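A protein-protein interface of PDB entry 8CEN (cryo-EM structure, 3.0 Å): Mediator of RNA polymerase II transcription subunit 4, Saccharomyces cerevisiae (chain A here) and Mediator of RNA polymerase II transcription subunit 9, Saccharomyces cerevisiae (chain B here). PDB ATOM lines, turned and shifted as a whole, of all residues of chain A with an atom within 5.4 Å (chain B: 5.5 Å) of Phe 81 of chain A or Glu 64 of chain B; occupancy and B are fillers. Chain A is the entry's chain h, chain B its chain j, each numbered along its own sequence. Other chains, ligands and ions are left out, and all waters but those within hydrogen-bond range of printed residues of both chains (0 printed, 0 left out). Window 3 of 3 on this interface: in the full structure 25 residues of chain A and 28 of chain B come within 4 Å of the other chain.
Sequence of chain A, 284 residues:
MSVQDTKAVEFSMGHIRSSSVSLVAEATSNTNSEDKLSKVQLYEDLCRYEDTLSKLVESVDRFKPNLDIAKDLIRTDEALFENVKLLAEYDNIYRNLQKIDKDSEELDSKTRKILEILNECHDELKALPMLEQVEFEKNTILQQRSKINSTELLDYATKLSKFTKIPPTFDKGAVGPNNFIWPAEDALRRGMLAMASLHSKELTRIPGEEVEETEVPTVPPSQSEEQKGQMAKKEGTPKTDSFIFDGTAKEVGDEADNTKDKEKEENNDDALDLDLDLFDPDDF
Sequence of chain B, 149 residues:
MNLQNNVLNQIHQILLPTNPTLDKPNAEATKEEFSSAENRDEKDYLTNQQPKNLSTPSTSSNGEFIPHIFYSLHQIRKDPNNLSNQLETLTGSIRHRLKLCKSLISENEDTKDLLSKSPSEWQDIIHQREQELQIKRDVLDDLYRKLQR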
ATOM      1  N   ASP A  77       8.798  24.108   2.254  1.00  0.00           N
ATOM      2  CA  ASP A  77       9.548  22.855   2.228  1.00  0.00           C
ATOM      3  C   ASP A  77       9.750  22.350   0.800  1.00  0.00           C
ATOM      4  O   ASP A  77      10.841  21.882   0.448  1.00  0.00           O
ATOM      5  CB  ASP A  77       8.828  21.804   3.077  1.00  0.00           C
ATOM      6  CG  ASP A  77       9.718  20.626   3.437  1.00  0.00           C
ATOM      7  OD1 ASP A  77      10.913  20.641   3.073  1.00  0.00           O
ATOM      8  OD2 ASP A  77       9.219  19.684   4.087  1.00  0.00           O
ATOM      9  N   GLU A  78       8.703  22.429  -0.028  1.00  0.00           N
ATOM     10  CA  GLU A  78       8.792  21.923  -1.397  1.00  0.00           C
ATOM     11  C   GLU A  78       9.771  22.742  -2.233  1.00  0.00           C
ATOM     12  O   GLU A  78      10.508  22.186  -3.058  1.00  0.00           O
ATOM     13  CB  GLU A  78       7.397  21.885  -2.036  1.00  0.00           C
ATOM     14  CG  GLU A  78       6.630  23.209  -2.081  1.00  0.00           C
ATOM     15  CD  GLU A  78       6.916  24.021  -3.332  1.00  0.00           C
ATOM     16  OE1 GLU A  78       7.393  23.434  -4.326  1.00  0.00           O
ATOM     17  OE2 GLU A  78       6.664  25.244  -3.320  1.00  0.00           O
ATOM     18  N   ALA A  79       9.807  24.060  -2.022  1.00  0.00           N
ATOM     19  CA  ALA A  79      10.779  24.886  -2.725  1.00  0.00           C
ATOM     20  C   ALA A  79      12.197  24.453  -2.385  1.00  0.00           C
ATOM     21  O   ALA A  79      13.034  24.306  -3.278  1.00  0.00           O
ATOM     22  CB  ALA A  79      10.560  26.361  -2.392  1.00  0.00           C
ATOM     23  N   LEU A  80      12.449  24.148  -1.108  1.00  0.00           N
ATOM     24  CA  LEU A  80      13.760  23.657  -0.691  1.00  0.00           C
ATOM     25  C   LEU A  80      14.089  22.300  -1.313  1.00  0.00           C
ATOM     26  O   LEU A  80      15.210  22.092  -1.793  1.00  0.00           O
ATOM     27  CB  LEU A  80      13.818  23.575   0.834  1.00  0.00           C
ATOM     28  CG  LEU A  80      15.069  22.956   1.460  1.00  0.00           C
ATOM     29  CD1 LEU A  80      16.295  23.803   1.161  1.00  0.00           C
ATOM     30  CD2 LEU A  80      14.884  22.788   2.960  1.00  0.00           C
ATOM     31  N   PHE A  81      13.130  21.368  -1.334  1.00  0.00           N
ATOM     32  CA  PHE A  81      13.460  20.019  -1.798  1.00  0.00           C
ATOM     33  C   PHE A  81      13.653  19.938  -3.314  1.00  0.00           C
ATOM     34  O   PHE A  81      14.647  19.362  -3.780  1.00  0.00           O
ATOM     35  CB  PHE A  81      12.406  19.016  -1.331  1.00  0.00           C
ATOM     36  CG  PHE A  81      12.549  18.623   0.114  1.00  0.00           C
ATOM     37  CD1 PHE A  81      13.766  18.770   0.764  1.00  0.00           C
ATOM     38  CD2 PHE A  81      11.483  18.078   0.813  1.00  0.00           C
ATOM     39  CE1 PHE A  81      13.913  18.405   2.090  1.00  0.00           C
ATOM     40  CE2 PHE A  81      11.625  17.705   2.139  1.00  0.00           C
ATOM     41  CZ  PHE A  81      12.841  17.872   2.779  1.00  0.00           C
ATOM     42  N   GLU A  82      12.748  20.509  -4.115  1.00  0.00           N
ATOM     43  CA  GLU A  82      13.079  20.561  -5.538  1.00  0.00           C
ATOM     44  C   GLU A  82      14.162  21.586  -5.882  1.00  0.00           C
ATOM     45  O   GLU A  82      14.766  21.466  -6.951  1.00  0.00           O
ATOM     46  CB  GLU A  82      11.836  20.729  -6.429  1.00  0.00           C
ATOM     47  CG  GLU A  82      10.910  19.479  -6.533  1.00  0.00           C
ATOM     48  CD  GLU A  82       9.901  19.255  -5.427  1.00  0.00           C
ATOM     49  OE1 GLU A  82       9.787  20.080  -4.519  1.00  0.00           O
ATOM     50  OE2 GLU A  82       9.204  18.220  -5.474  1.00  0.00           O
ATOM     51  N   ASN A  83      14.512  22.517  -4.989  1.00  0.00           N
ATOM     52  CA  ASN A  83      15.739  23.274  -5.218  1.00  0.00           C
ATOM     53  C   ASN A  83      16.974  22.408  -4.996  1.00  0.00           C
ATOM     54  O   ASN A  83      17.978  22.581  -5.692  1.00  0.00           O
ATOM     55  CB  ASN A  83      15.780  24.513  -4.325  1.00  0.00           C
ATOM     56  CG  ASN A  83      15.175  25.733  -4.994  1.00  0.00           C
ATOM     57  OD1 ASN A  83      14.416  25.614  -5.957  1.00  0.00           O
ATOM     58  ND2 ASN A  83      15.509  26.914  -4.487  1.00  0.00           N
ATOM     59  N   VAL A  84      16.913  21.468  -4.052  1.00  0.00           N
ATOM     60  CA  VAL A  84      17.989  20.493  -3.885  1.00  0.00           C
ATOM     61  C   VAL A  84      18.090  19.593  -5.117  1.00  0.00           C
ATOM     62  O   VAL A  84      19.192  19.273  -5.585  1.00  0.00           O
ATOM     63  CB  VAL A  84      17.769  19.686  -2.589  1.00  0.00           C
ATOM     64  CG1 VAL A  84      18.610  18.416  -2.566  1.00  0.00           C
ATOM     65  CG2 VAL A  84      18.083  20.546  -1.375  1.00  0.00           C
ATOM     66  N   LYS A  85      16.943  19.185  -5.667  1.00  0.00           N
ATOM     67  CA  LYS A  85      16.949  18.378  -6.889  1.00  0.00           C
ATOM     68  C   LYS A  85      17.533  19.150  -8.074  1.00  0.00           C
ATOM     69  O   LYS A  85      18.341  18.613  -8.847  1.00  0.00           O
ATOM     70  CB  LYS A  85      15.535  17.893  -7.206  1.00  0.00           C
ATOM     71  CG  LYS A  85      15.249  16.470  -6.747  1.00  0.00           C
ATOM     72  CD  LYS A  85      14.998  16.407  -5.249  1.00  0.00           C
ATOM     73  CE  LYS A  85      14.927  14.968  -4.759  1.00  0.00           C
ATOM     74  NZ  LYS A  85      14.332  14.869  -3.397  1.00  0.00           N
ATOM     75  N   LEU A  86      17.163  20.422  -8.226  1.00  0.00           N
ATOM     76  CA  LEU A  86      17.764  21.205  -9.298  1.00  0.00           C
ATOM     77  C   LEU A  86      19.209  21.594  -8.995  1.00  0.00           C
ATOM     78  O   LEU A  86      19.945  21.934  -9.920  1.00  0.00           O
ATOM     79  CB  LEU A  86      16.922  22.444  -9.615  1.00  0.00           C
ATOM     80  CG  LEU A  86      15.754  22.274 -10.608  1.00  0.00           C
ATOM     81  CD1 LEU A  86      16.288  21.870 -11.979  1.00  0.00           C
ATOM     82  CD2 LEU A  86      14.654  21.311 -10.168  1.00  0.00           C
ATOM     83  N   LEU B  15      22.957  18.947   4.083  1.00  0.00           N
ATOM     84  CA  LEU B  15      21.561  19.363   4.109  1.00  0.00           C
ATOM     85  C   LEU B  15      20.600  18.186   4.034  1.00  0.00           C
ATOM     86  O   LEU B  15      19.526  18.233   4.646  1.00  0.00           O
ATOM     87  CB  LEU B  15      21.278  20.325   2.950  1.00  0.00           C
ATOM     88  CG  LEU B  15      20.017  21.185   3.053  1.00  0.00           C
ATOM     89  CD1 LEU B  15      20.132  22.162   4.210  1.00  0.00           C
ATOM     90  CD2 LEU B  15      19.756  21.920   1.747  1.00  0.00           C
ATOM     91  N   LEU B  16      20.960  17.133   3.301  1.00  0.00           N
ATOM     92  CA  LEU B  16      20.138  15.935   3.143  1.00  0.00           C
ATOM     93  C   LEU B  16      20.995  14.732   3.512  1.00  0.00           C
ATOM     94  O   LEU B  16      21.584  14.084   2.636  1.00  0.00           O
ATOM     95  CB  LEU B  16      19.599  15.805   1.716  1.00  0.00           C
ATOM     96  CG  LEU B  16      18.267  16.451   1.314  1.00  0.00           C
ATOM     97  CD1 LEU B  16      17.124  15.867   2.128  1.00  0.00           C
ATOM     98  CD2 LEU B  16      18.289  17.972   1.416  1.00  0.00           C
ATOM     99  N   PRO B  17      21.108  14.420   4.803  1.00  0.00           N
ATOM    100  CA  PRO B  17      21.940  13.283   5.215  1.00  0.00           C
ATOM    101  C   PRO B  17      21.336  11.954   4.791  1.00  0.00           C
ATOM    102  O   PRO B  17      20.116  11.802   4.677  1.00  0.00           O
ATOM    103  CB  PRO B  17      21.985  13.412   6.742  1.00  0.00           C
ATOM    104  CG  PRO B  17      20.727  14.127   7.091  1.00  0.00           C
ATOM    105  CD  PRO B  17      20.430  15.058   5.945  1.00  0.00           C
ATOM    106  N   ASN B  62      19.146  10.679   7.933  1.00  0.00           N
ATOM    107  CA  ASN B  62      18.780  10.881   9.330  1.00  0.00           C
ATOM    108  C   ASN B  62      17.767  12.013   9.469  1.00  0.00           C
ATOM    109  O   ASN B  62      17.040  12.325   8.527  1.00  0.00           O
ATOM    110  CB  ASN B  62      20.022  11.178  10.173  1.00  0.00           C
ATOM    111  CG  ASN B  62      21.146  10.193   9.920  1.00  0.00           C
ATOM    112  OD1 ASN B  62      21.061   9.025  10.297  1.00  0.00           O
ATOM    113  ND2 ASN B  62      22.210  10.663   9.280  1.00  0.00           N
ATOM    114  N   GLY B  63      17.725  12.622  10.652  1.00  0.00           N
ATOM    115  CA  GLY B  63      16.831  13.736  10.899  1.00  0.00           C
ATOM    116  C   GLY B  63      17.233  14.989  10.150  1.00  0.00           C
ATOM    117  O   GLY B  63      18.271  15.588  10.448  1.00  0.00           O
ATOM    118  N   GLU B  64      16.423  15.400   9.171  1.00  0.00           N
ATOM    119  CA  GLU B  64      16.801  16.536   8.333  1.00  0.00           C
ATOM    120  C   GLU B  64      16.491  17.878   9.006  1.00  0.00           C
ATOM    121  O   GLU B  64      17.408  18.633   9.342  1.00  0.00           O
ATOM    122  CB  GLU B  64      16.153  16.385   6.945  1.00  0.00           C
ATOM    123  CG  GLU B  64      14.632  16.154   6.902  1.00  0.00           C
ATOM    124  CD  GLU B  64      14.112  15.868   5.509  1.00  0.00           C
ATOM    125  OE1 GLU B  64      14.928  15.812   4.568  1.00  0.00           O
ATOM    126  OE2 GLU B  64      12.885  15.697   5.357  1.00  0.00           O
ATOM    127  N   PHE B  65      15.216  18.197   9.213  1.00  0.00           N
ATOM    128  CA  PHE B  65      14.838  19.322  10.060  1.00  0.00           C
ATOM    129  C   PHE B  65      13.720  18.978  11.032  1.00  0.00           C
ATOM    130  O   PHE B  65      13.780  19.373  12.199  1.00  0.00           O
ATOM    131  CB  PHE B  65      14.409  20.511   9.185  1.00  0.00           C
ATOM    132  CG  PHE B  65      15.514  21.070   8.337  1.00  0.00           C
ATOM    133  CD1 PHE B  65      16.393  22.008   8.848  1.00  0.00           C
ATOM    134  CD2 PHE B  65      15.668  20.657   7.022  1.00  0.00           C
ATOM    135  CE1 PHE B  65      17.409  22.523   8.063  1.00  0.00           C
ATOM    136  CE2 PHE B  65      16.682  21.168   6.234  1.00  0.00           C
ATOM    137  CZ  PHE B  65      17.553  22.102   6.756  1.00  0.00           C
ATOM    138  N   ILE B  66      12.707  18.247  10.576  1.00  0.00           N
ATOM    139  CA  ILE B  66      11.554  17.852  11.385  1.00  0.00           C
ATOM    140  C   ILE B  66      11.729  16.621  12.285  1.00  0.00           C
ATOM    141  O   ILE B  66      11.097  16.615  13.352  1.00  0.00           O
ATOM    142  CB  ILE B  66      10.299  17.701  10.500  1.00  0.00           C
ATOM    143  CG1 ILE B  66      10.489  16.677   9.380  1.00  0.00           C
ATOM    144  CG2 ILE B  66       9.900  19.050   9.914  1.00  0.00           C
ATOM    145  CD1 ILE B  66       9.256  16.466   8.526  1.00  0.00           C
ATOM    146  N   PRO B  67      12.471  15.546  11.930  1.00  0.00           N
ATOM    147  CA  PRO B  67      12.420  14.358  12.807  1.00  0.00           C
ATOM    148  C   PRO B  67      13.028  14.586  14.174  1.00  0.00           C
ATOM    149  O   PRO B  67      12.477  14.111  15.176  1.00  0.00           O
ATOM    150  CB  PRO B  67      13.193  13.295  12.012  1.00  0.00           C
ATOM    151  CG  PRO B  67      13.192  13.792  10.625  1.00  0.00           C
ATOM    152  CD  PRO B  67      13.375  15.249  10.801  1.00  0.00           C
ATOM    153  N   ILE B  94      21.417  21.556  15.392  1.00  0.00           N
ATOM    154  CA  ILE B  94      20.858  21.734  14.055  1.00  0.00           C
ATOM    155  C   ILE B  94      21.024  23.179  13.591  1.00  0.00           C
ATOM    156  O   ILE B  94      21.309  23.439  12.418  1.00  0.00           O
ATOM    157  CB  ILE B  94      19.383  21.294  14.032  1.00  0.00           C
ATOM    158  CG1 ILE B  94      19.225  19.903  14.654  1.00  0.00           C
ATOM    159  CG2 ILE B  94      18.839  21.298  12.610  1.00  0.00           C
ATOM    160  CD1 ILE B  94      19.999  18.813  13.937  1.00  0.00           C
ATOM    161  N   ARG B  97      24.369  23.586  12.483  1.00  0.00           N
ATOM    162  CA  ARG B  97      24.457  22.994  11.150  1.00  0.00           C
ATOM    163  C   ARG B  97      23.957  23.965  10.081  1.00  0.00           C
ATOM    164  O   ARG B  97      24.512  24.021   8.979  1.00  0.00           O
ATOM    165  CB  ARG B  97      23.678  21.675  11.118  1.00  0.00           C
ATOM    166  CG  ARG B  97      23.432  21.086   9.737  1.00  0.00           C
ATOM    167  CD  ARG B  97      22.245  20.134   9.759  1.00  0.00           C
ATOM    168  NE  ARG B  97      22.547  18.903  10.479  1.00  0.00           N
ATOM    169  CZ  ARG B  97      21.717  17.875  10.589  1.00  0.00           C
ATOM    170  NH1 ARG B  97      20.512  17.898  10.041  1.00  0.00           N
ATOM    171  NH2 ARG B  97      22.103  16.797  11.265  1.00  0.00           N
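NH1 of Arg 97 of chain B is in hydrogen-bond range of O of Glu 64 of chain B (3.3 Å).
Leu 15 of chain B touches Leu 80 of chain A.
Glu 64 of chain B touches Phe 81 of chain A.
Val 84 of chain A touches Leu 15 of chain B.
CD2 of Leu 16 of chain B touches CG2 of Val 84 of chain A, at 3.8 Å.
Of chain B, only Glu 64 (3.4 Å) comes within 4 Å of Phe 81 of chain A.
Of the printed residues of chain B, Val 84 of chain A touches Leu 15 (3.8 Å) and Leu 16 (3.8 Å).
Printed residues of chain B within 4 Å of Leu 80 of chain A: Leu 15.
Of the printed residues of chain A, Leu 16 of chain B touches Val 84 (3.8 Å).
Of the printed residues of chain A, Leu 15 of chain B touches Leu 80 (3.98 Å) and Val 84 (3.8 Å).
The nearest residue of chain B that does not touch Phe 81 of chain A is Leu 16 of chain B (4.1 Å).
Of the 10 printed residues of chain A, 3 touch a printed residue of chain B.
Of the 11 printed residues of chain B, 3 touch a printed residue of chain A.
Among the printed residues, no Asp or Glu carboxylate lies within 4 Å of a Lys or Arg side-chain nitrogen of the other chain.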
